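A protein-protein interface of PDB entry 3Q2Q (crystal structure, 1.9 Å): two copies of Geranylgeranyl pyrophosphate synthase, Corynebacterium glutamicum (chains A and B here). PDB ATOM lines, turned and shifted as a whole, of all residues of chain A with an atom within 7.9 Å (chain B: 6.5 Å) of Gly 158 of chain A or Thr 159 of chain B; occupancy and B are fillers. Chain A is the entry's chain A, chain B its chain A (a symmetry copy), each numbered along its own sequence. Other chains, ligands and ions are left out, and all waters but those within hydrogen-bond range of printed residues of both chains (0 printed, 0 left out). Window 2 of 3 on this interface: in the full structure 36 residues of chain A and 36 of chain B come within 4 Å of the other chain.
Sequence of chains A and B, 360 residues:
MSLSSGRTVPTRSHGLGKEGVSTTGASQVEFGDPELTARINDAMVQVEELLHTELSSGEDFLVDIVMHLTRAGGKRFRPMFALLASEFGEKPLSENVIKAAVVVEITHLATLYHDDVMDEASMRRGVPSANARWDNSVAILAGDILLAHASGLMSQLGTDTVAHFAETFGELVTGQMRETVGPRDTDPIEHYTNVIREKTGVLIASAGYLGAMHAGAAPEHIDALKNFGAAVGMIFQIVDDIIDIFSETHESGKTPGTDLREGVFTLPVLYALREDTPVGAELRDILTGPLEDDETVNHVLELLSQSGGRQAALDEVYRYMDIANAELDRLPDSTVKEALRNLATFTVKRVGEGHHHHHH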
ATOM      1  N   ASN A  96      21.688 -31.168  -1.022  1.00  0.00           N
ATOM      2  CA  ASN A  96      22.190 -29.791  -1.136  1.00  0.00           C
ATOM      3  C   ASN A  96      22.847 -29.486  -2.493  1.00  0.00           C
ATOM      4  O   ASN A  96      22.875 -28.333  -2.940  1.00  0.00           O
ATOM      5  CB  ASN A  96      23.129 -29.448   0.011  1.00  0.00           C
ATOM      6  CG  ASN A  96      22.389 -29.219   1.322  1.00  0.00           C
ATOM      7  OD1 ASN A  96      21.153 -29.195   1.363  1.00  0.00           O
ATOM      8  ND2 ASN A  96      23.144 -29.037   2.401  1.00  0.00           N
ATOM      9  N   SER A 151      17.105 -16.909  -3.419  1.00  0.00           N
ATOM     10  CA  SER A 151      17.629 -16.526  -2.106  1.00  0.00           C
ATOM     11  C   SER A 151      17.083 -17.391  -0.976  1.00  0.00           C
ATOM     12  O   SER A 151      17.805 -17.682   0.005  1.00  0.00           O
ATOM     13  CB  SER A 151      17.345 -15.046  -1.813  1.00  0.00           C
ATOM     14  OG  SER A 151      18.010 -14.242  -2.765  1.00  0.00           O
ATOM     15  N   GLY A 152      15.816 -17.784  -1.083  1.00  0.00           N
ATOM     16  CA  GLY A 152      15.234 -18.704  -0.103  1.00  0.00           C
ATOM     17  C   GLY A 152      16.064 -19.979   0.003  1.00  0.00           C
ATOM     18  O   GLY A 152      16.448 -20.403   1.100  1.00  0.00           O
ATOM     19  N   LEU A 153      16.333 -20.606  -1.136  1.00  0.00           N
ATOM     20  CA  LEU A 153      17.152 -21.828  -1.141  1.00  0.00           C
ATOM     21  C   LEU A 153      18.579 -21.599  -0.623  1.00  0.00           C
ATOM     22  O   LEU A 153      19.086 -22.399   0.162  1.00  0.00           O
ATOM     23  CB  LEU A 153      17.195 -22.446  -2.540  1.00  0.00           C
ATOM     24  CG  LEU A 153      15.855 -22.953  -3.057  1.00  0.00           C
ATOM     25  CD1 LEU A 153      15.991 -23.378  -4.506  1.00  0.00           C
ATOM     26  CD2 LEU A 153      15.338 -24.108  -2.193  1.00  0.00           C
ATOM     27  N   MET A 154      19.208 -20.499  -1.040  1.00  0.00           N
ATOM     28  CA  MET A 154      20.565 -20.200  -0.586  1.00  0.00           C
ATOM     29  C   MET A 154      20.634 -20.038   0.923  1.00  0.00           C
ATOM     30  O   MET A 154      21.669 -20.342   1.527  1.00  0.00           O
ATOM     31  CB  MET A 154      21.109 -18.945  -1.259  1.00  0.00           C
ATOM     32  CG  MET A 154      21.435 -19.139  -2.719  1.00  0.00           C
ATOM     33  SD  MET A 154      22.403 -17.784  -3.406  1.00  0.00           S
ATOM     34  CE  MET A 154      22.128 -16.471  -2.228  1.00  0.00           C
ATOM     35  N   SER A 155      19.550 -19.581   1.534  1.00  0.00           N
ATOM     36  CA  SER A 155      19.541 -19.428   2.991  1.00  0.00           C
ATOM     37  C   SER A 155      19.678 -20.783   3.663  1.00  0.00           C
ATOM     38  O   SER A 155      20.035 -20.865   4.826  1.00  0.00           O
ATOM     39  CB  SER A 155      18.270 -18.732   3.512  1.00  0.00           C
ATOM     40  OG  SER A 155      17.124 -19.584   3.539  1.00  0.00           O
ATOM     41  N   GLN A 156      19.372 -21.848   2.936  1.00  0.00           N
ATOM     42  CA  GLN A 156      19.503 -23.169   3.528  1.00  0.00           C
ATOM     43  C   GLN A 156      20.847 -23.786   3.163  1.00  0.00           C
ATOM     44  O   GLN A 156      21.222 -24.832   3.706  1.00  0.00           O
ATOM     45  CB  GLN A 156      18.355 -24.080   3.095  1.00  0.00           C
ATOM     46  CG  GLN A 156      16.976 -23.643   3.581  1.00  0.00           C
ATOM     47  CD  GLN A 156      15.871 -24.614   3.141  1.00  0.00           C
ATOM     48  OE1 GLN A 156      15.729 -24.932   1.953  1.00  0.00           O
ATOM     49  NE2 GLN A 156      15.101 -25.095   4.105  1.00  0.00           N
ATOM     50  N   LEU A 157      21.575 -23.137   2.258  1.00  0.00           N
ATOM     51  CA  LEU A 157      22.841 -23.669   1.751  1.00  0.00           C
ATOM     52  C   LEU A 157      24.068 -23.117   2.485  1.00  0.00           C
ATOM     53  O   LEU A 157      25.159 -23.673   2.386  1.00  0.00           O
ATOM     54  CB  LEU A 157      22.963 -23.438   0.232  1.00  0.00           C
ATOM     55  CG  LEU A 157      22.031 -24.348  -0.592  1.00  0.00           C
ATOM     56  CD1 LEU A 157      22.109 -23.998  -2.062  1.00  0.00           C
ATOM     57  CD2 LEU A 157      22.372 -25.846  -0.365  1.00  0.00           C
ATOM     58  N   GLY A 158      23.893 -22.013   3.205  1.00  0.00           N
ATOM     59  CA  GLY A 158      24.987 -21.436   3.975  1.00  0.00           C
ATOM     60  C   GLY A 158      25.494 -20.110   3.427  1.00  0.00           C
ATOM     61  O   GLY A 158      25.310 -19.786   2.250  1.00  0.00           O
ATOM     62  N   THR A 159      26.150 -19.343   4.284  1.00  0.00           N
ATOM     63  CA  THR A 159      26.612 -18.006   3.907  1.00  0.00           C
ATOM     64  C   THR A 159      27.697 -18.019   2.820  1.00  0.00           C
ATOM     65  O   THR A 159      27.788 -17.068   2.036  1.00  0.00           O
ATOM     66  CB  THR A 159      27.136 -17.211   5.144  1.00  0.00           C
ATOM     67  OG1 THR A 159      28.214 -17.929   5.734  1.00  0.00           O
ATOM     68  CG2 THR A 159      26.052 -17.029   6.170  1.00  0.00           C
ATOM     69  N   ASP A 160      28.523 -19.065   2.753  1.00  0.00           N
ATOM     70  CA  ASP A 160      29.548 -19.134   1.729  1.00  0.00           C
ATOM     71  C   ASP A 160      28.896 -19.178   0.337  1.00  0.00           C
ATOM     72  O   ASP A 160      29.410 -18.619  -0.609  1.00  0.00           O
ATOM     73  CB  ASP A 160      30.442 -20.357   1.951  1.00  0.00           C
ATOM     74  CG  ASP A 160      31.255 -20.271   3.244  1.00  0.00           C
ATOM     75  OD1 ASP A 160      31.470 -19.150   3.762  1.00  0.00           O
ATOM     76  OD2 ASP A 160      31.685 -21.334   3.740  1.00  0.00           O
ATOM     77  N   THR A 161      27.768 -19.881   0.237  1.00  0.00           N
ATOM     78  CA  THR A 161      27.021 -19.939  -1.019  1.00  0.00           C
ATOM     79  C   THR A 161      26.448 -18.570  -1.360  1.00  0.00           C
ATOM     80  O   THR A 161      26.489 -18.140  -2.524  1.00  0.00           O
ATOM     81  CB  THR A 161      25.899 -20.940  -0.908  1.00  0.00           C
ATOM     82  OG1 THR A 161      26.466 -22.252  -0.881  1.00  0.00           O
ATOM     83  CG2 THR A 161      24.947 -20.821  -2.104  1.00  0.00           C
ATOM     84  N   VAL A 162      25.923 -17.885  -0.340  1.00  0.00           N
ATOM     85  CA  VAL A 162      25.342 -16.543  -0.537  1.00  0.00           C
ATOM     86  C   VAL A 162      26.434 -15.555  -0.999  1.00  0.00           C
ATOM     87  O   VAL A 162      26.237 -14.808  -1.948  1.00  0.00           O
ATOM     88  CB  VAL A 162      24.633 -16.017   0.723  1.00  0.00           C
ATOM     89  CG1 VAL A 162      24.067 -14.584   0.488  1.00  0.00           C
ATOM     90  CG2 VAL A 162      23.488 -17.001   1.174  1.00  0.00           C
ATOM     91  N   ALA A 163      27.577 -15.563  -0.319  1.00  0.00           N
ATOM     92  CA  ALA A 163      28.742 -14.765  -0.719  1.00  0.00           C
ATOM     93  C   ALA A 163      29.169 -15.071  -2.154  1.00  0.00           C
ATOM     94  O   ALA A 163      29.370 -14.154  -2.975  1.00  0.00           O
ATOM     95  CB  ALA A 163      29.909 -15.013   0.237  1.00  0.00           C
ATOM     96  N   HIS A 164      29.328 -16.364  -2.459  1.00  0.00           N
ATOM     97  CA  HIS A 164      29.720 -16.766  -3.801  1.00  0.00           C
ATOM     98  C   HIS A 164      28.685 -16.324  -4.830  1.00  0.00           C
ATOM     99  O   HIS A 164      29.030 -15.914  -5.946  1.00  0.00           O
ATOM    100  CB  HIS A 164      29.867 -18.294  -3.880  1.00  0.00           C
ATOM    101  CG  HIS A 164      29.948 -18.799  -5.288  1.00  0.00           C
ATOM    102  ND1 HIS A 164      31.121 -18.809  -6.009  1.00  0.00           N
ATOM    103  CD2 HIS A 164      28.985 -19.250  -6.129  1.00  0.00           C
ATOM    104  CE1 HIS A 164      30.884 -19.268  -7.228  1.00  0.00           C
ATOM    105  NE2 HIS A 164      29.596 -19.542  -7.324  1.00  0.00           N
ATOM    106  N   PHE A 165      27.412 -16.429  -4.456  1.00  0.00           N
ATOM    107  CA  PHE A 165      26.331 -16.053  -5.344  1.00  0.00           C
ATOM    108  C   PHE A 165      26.364 -14.570  -5.572  1.00  0.00           C
ATOM    109  O   PHE A 165      26.163 -14.091  -6.678  1.00  0.00           O
ATOM    110  CB  PHE A 165      24.950 -16.409  -4.763  1.00  0.00           C
ATOM    111  CG  PHE A 165      23.804 -15.647  -5.420  1.00  0.00           C
ATOM    112  CD1 PHE A 165      23.187 -16.138  -6.569  1.00  0.00           C
ATOM    113  CD2 PHE A 165      23.370 -14.419  -4.906  1.00  0.00           C
ATOM    114  CE1 PHE A 165      22.133 -15.427  -7.184  1.00  0.00           C
ATOM    115  CE2 PHE A 165      22.330 -13.700  -5.518  1.00  0.00           C
ATOM    116  CZ  PHE A 165      21.707 -14.208  -6.661  1.00  0.00           C
ATOM    117  N   LEU A 210      29.745 -24.777  -6.969  1.00  0.00           N
ATOM    118  CA  LEU A 210      28.747 -25.115  -5.987  1.00  0.00           C
ATOM    119  C   LEU A 210      28.485 -26.624  -5.959  1.00  0.00           C
ATOM    120  O   LEU A 210      28.284 -27.192  -4.902  1.00  0.00           O
ATOM    121  CB  LEU A 210      27.454 -24.346  -6.248  1.00  0.00           C
ATOM    122  CG  LEU A 210      27.556 -22.836  -5.949  1.00  0.00           C
ATOM    123  CD1 LEU A 210      26.248 -22.131  -6.407  1.00  0.00           C
ATOM    124  CD2 LEU A 210      27.853 -22.595  -4.451  1.00  0.00           C
ATOM    125  N   MET A 213      31.508 -28.059  -4.121  1.00  0.00           N
ATOM    126  CA  MET A 213      31.555 -27.634  -2.724  1.00  0.00           C
ATOM    127  C   MET A 213      30.481 -28.313  -1.861  1.00  0.00           C
ATOM    128  O   MET A 213      30.782 -28.842  -0.786  1.00  0.00           O
ATOM    129  CB  MET A 213      31.477 -26.111  -2.620  1.00  0.00           C
ATOM    130  CG  MET A 213      31.721 -25.579  -1.219  1.00  0.00           C
ATOM    131  SD  MET A 213      30.193 -25.384  -0.286  1.00  0.00           S
ATOM    132  CE  MET A 213      29.581 -23.848  -0.987  1.00  0.00           C
ATOM    133  N   HIS A 214      29.236 -28.311  -2.321  1.00  0.00           N
ATOM    134  CA  HIS A 214      28.168 -28.985  -1.572  1.00  0.00           C
ATOM    135  C   HIS A 214      28.222 -30.523  -1.589  1.00  0.00           C
ATOM    136  O   HIS A 214      27.443 -31.176  -0.903  1.00  0.00           O
ATOM    137  CB  HIS A 214      26.788 -28.486  -1.993  1.00  0.00           C
ATOM    138  CG  HIS A 214      26.515 -27.095  -1.528  1.00  0.00           C
ATOM    139  ND1 HIS A 214      26.235 -26.799  -0.212  1.00  0.00           N
ATOM    140  CD2 HIS A 214      26.592 -25.908  -2.175  1.00  0.00           C
ATOM    141  CE1 HIS A 214      26.088 -25.490  -0.078  1.00  0.00           C
ATOM    142  NE2 HIS A 214      26.300 -24.927  -1.255  1.00  0.00           N
ATOM    143  N   MET B 154      24.469  -9.336   3.148  1.00  0.00           N
ATOM    144  CA  MET B 154      23.697 -10.349   3.864  1.00  0.00           C
ATOM    145  C   MET B 154      24.518 -11.598   4.135  1.00  0.00           C
ATOM    146  O   MET B 154      24.289 -12.278   5.142  1.00  0.00           O
ATOM    147  CB  MET B 154      22.434 -10.725   3.099  1.00  0.00           C
ATOM    148  CG  MET B 154      21.381  -9.644   3.106  1.00  0.00           C
ATOM    149  SD  MET B 154      19.779 -10.225   2.524  1.00  0.00           S
ATOM    150  CE  MET B 154      20.201 -11.717   1.639  1.00  0.00           C
ATOM    151  N   SER B 155      25.472 -11.897   3.265  1.00  0.00           N
ATOM    152  CA  SER B 155      26.320 -13.073   3.483  1.00  0.00           C
ATOM    153  C   SER B 155      27.149 -12.898   4.743  1.00  0.00           C
ATOM    154  O   SER B 155      27.649 -13.863   5.295  1.00  0.00           O
ATOM    155  CB  SER B 155      27.258 -13.363   2.297  1.00  0.00           C
ATOM    156  OG  SER B 155      28.388 -12.491   2.238  1.00  0.00           O
ATOM    157  N   LEU B 157      25.856 -11.282   7.357  1.00  0.00           N
ATOM    158  CA  LEU B 157      24.868 -11.090   8.420  1.00  0.00           C
ATOM    159  C   LEU B 157      24.264 -12.403   8.931  1.00  0.00           C
ATOM    160  O   LEU B 157      23.657 -12.438   9.998  1.00  0.00           O
ATOM    161  CB  LEU B 157      23.761 -10.118   7.968  1.00  0.00           C
ATOM    162  CG  LEU B 157      24.241  -8.655   7.888  1.00  0.00           C
ATOM    163  CD1 LEU B 157      23.149  -7.767   7.331  1.00  0.00           C
ATOM    164  CD2 LEU B 157      24.708  -8.144   9.278  1.00  0.00           C
ATOM    165  N   GLY B 158      24.413 -13.475   8.160  1.00  0.00           N
ATOM    166  CA  GLY B 158      23.914 -14.778   8.578  1.00  0.00           C
ATOM    167  C   GLY B 158      22.727 -15.273   7.766  1.00  0.00           C
ATOM    168  O   GLY B 158      22.006 -14.493   7.135  1.00  0.00           O
ATOM    169  N   THR B 159      22.511 -16.579   7.792  1.00  0.00           N
ATOM    170  CA  THR B 159      21.457 -17.192   6.983  1.00  0.00           C
ATOM    171  C   THR B 159      20.041 -16.776   7.408  1.00  0.00           C
ATOM    172  O   THR B 159      19.137 -16.733   6.567  1.00  0.00           O
ATOM    173  CB  THR B 159      21.558 -18.749   6.994  1.00  0.00           C
ATOM    174  OG1 THR B 159      21.445 -19.211   8.336  1.00  0.00           O
ATOM    175  CG2 THR B 159      22.871 -19.212   6.428  1.00  0.00           C
ATOM    176  N   ASP B 160      19.822 -16.470   8.689  1.00  0.00           N
ATOM    177  CA  ASP B 160      18.508 -16.049   9.136  1.00  0.00           C
ATOM    178  C   ASP B 160      18.118 -14.732   8.442  1.00  0.00           C
ATOM    179  O   ASP B 160      16.968 -14.515   8.119  1.00  0.00           O
ATOM    180  CB  ASP B 160      18.486 -15.891  10.658  1.00  0.00           C
ATOM    181  CG  ASP B 160      18.687 -17.216  11.394  1.00  0.00           C
ATOM    182  OD1 ASP B 160      18.437 -18.293  10.803  1.00  0.00           O
ATOM    183  OD2 ASP B 160      19.096 -17.177  12.574  1.00  0.00           O
ATOM    184  N   THR B 161      19.100 -13.852   8.253  1.00  0.00           N
ATOM    185  CA  THR B 161      18.866 -12.594   7.546  1.00  0.00           C
ATOM    186  C   THR B 161      18.537 -12.861   6.082  1.00  0.00           C
ATOM    187  O   THR B 161      17.629 -12.233   5.514  1.00  0.00           O
ATOM    188  CB  THR B 161      20.087 -11.714   7.633  1.00  0.00           C
ATOM    189  OG1 THR B 161      20.205 -11.239   8.977  1.00  0.00           O
ATOM    190  CG2 THR B 161      19.964 -10.521   6.680  1.00  0.00           C
ATOM    191  N   VAL B 162      19.271 -13.802   5.481  1.00  0.00           N
ATOM    192  CA  VAL B 162      19.046 -14.159   4.066  1.00  0.00           C
ATOM    193  C   VAL B 162      17.634 -14.757   3.889  1.00  0.00           C
ATOM    194  O   VAL B 162      16.905 -14.372   2.985  1.00  0.00           O
ATOM    195  CB  VAL B 162      20.116 -15.125   3.527  1.00  0.00           C
ATOM    196  CG1 VAL B 162      19.823 -15.510   2.045  1.00  0.00           C
ATOM    197  CG2 VAL B 162      21.555 -14.502   3.667  1.00  0.00           C
ATOM    198  N   ALA B 163      17.265 -15.695   4.757  1.00  0.00           N
ATOM    199  CA  ALA B 163      15.913 -16.263   4.782  1.00  0.00           C
ATOM    200  C   ALA B 163      14.848 -15.179   4.941  1.00  0.00           C
ATOM    201  O   ALA B 163      13.858 -15.132   4.185  1.00  0.00           O
ATOM    202  CB  ALA B 163      15.788 -17.288   5.909  1.00  0.00           C
ATOM    203  N   HIS B 164      15.037 -14.311   5.941  1.00  0.00           N
ATOM    204  CA  HIS B 164      14.090 -13.230   6.174  1.00  0.00           C
ATOM    205  C   HIS B 164      14.005 -12.306   4.966  1.00  0.00           C
ATOM    206  O   HIS B 164      12.925 -11.817   4.610  1.00  0.00           O
ATOM    207  CB  HIS B 164      14.514 -12.401   7.397  1.00  0.00           C
ATOM    208  CG  HIS B 164      13.781 -11.099   7.499  1.00  0.00           C
ATOM    209  ND1 HIS B 164      12.528 -10.992   8.061  1.00  0.00           N
ATOM    210  CD2 HIS B 164      14.099  -9.860   7.051  1.00  0.00           C
ATOM    211  CE1 HIS B 164      12.115  -9.738   7.980  1.00  0.00           C
ATOM    212  NE2 HIS B 164      13.050  -9.033   7.370  1.00  0.00           N
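OG of Ser 155 of chain A is in hydrogen-bond range of O of Gly 152 of chain A (2.7 Å).
Among the printed residues, pairs that only touch across the chains: Thr 159 of chain A with Ser 155 of chain B (3.4 Å), Ser 155 of chain A with Thr 159 of chain B (3.4 Å), Ser 155 of chain A with Ala 163 of chain B (3.4 Å), Ala 163 of chain A with Ser 155 of chain B (3.4 Å), Ser 151 of chain A with Val 162 of chain B (3.6 Å), Ser 155 of chain A with Val 162 of chain B (3.9 Å), Val 162 of chain A with Ser 155 of chain B (3.9 Å), Thr 159 of chain A with Thr 159 of chain B (3.9 Å), Thr 159 of chain A with Gly 158 of chain B (3.9 Å) and Gly 158 of chain A with Thr 159 of chain B (3.9 Å).
Printed residues of chain B within 4 Å of Ser 151 of chain A: Val 162. Gln 156 of chain A touches none of the printed residues of chain B. Of the printed residues of chain B, Thr 159 of chain A touches Ser 155, Gly 158 and Thr 159. Of chain A, only Ser 155 (3.4 Å), Gly 158 (3.9 Å) and Thr 159 (3.9 Å) come within 4 Å of Thr 159 of chain B. Asp 160 of chain B touches none of the printed residues of chain A. Of the printed residues of chain A, Ala 163 of chain B touches Ser 155. The nearest printed residue of chain B that does not touch Gly 158 of chain A is Val 162 of chain B (6.6 Å). The nearest printed residue of chain A that does not touch Thr 159 of chain B is Met 154 of chain A (5.2 Å).
Printed residues of chain B that touch a printed residue of chain A: Ser 155, Gly 158, Thr 159, Val 162 and Ala 163. Hydrophobic or aromatic side chains of chain B within 4 Å of the printed part of chain A: Val 162 and Ala 163. Printed residues of chain A that touch a printed residue of chain B: Ser 151, Ser 155, Gly 158, Thr 159, Val 162 and Ala 163. Hydrophobic or aromatic side chains of chain A within 4 Å of the printed part of chain B: Val 162 and Ala 163. Among the printed residues, no Asp or Glu carboxylate lies within 4 Å of a Lys or Arg side-chain nitrogen of the other chain.
Ser 155 of chain A touches Thr 159 of chain B, and with the chains exchanged Thr 159 of chain A touches Ser 155 of chain B. Ser 155 of chain A touches Val 162 of chain B, and with the chains exchanged Val 162 of chain A touches Ser 155 of chain B. Gly 158 of chain A touches Thr 159 of chain B, and with the chains exchanged Thr 159 of chain A touches Gly 158 of chain B. Thr 159 of chain B touches its own counterpart, Thr 159 of chain A. Positions printed for both chains: 154, 155, 157, 158, 159, 160, 161, 162, 163 and 164. Of the 10 pairs that touch across the chains among the printed residues, 9 have their exchanged pair printed and touching as well.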
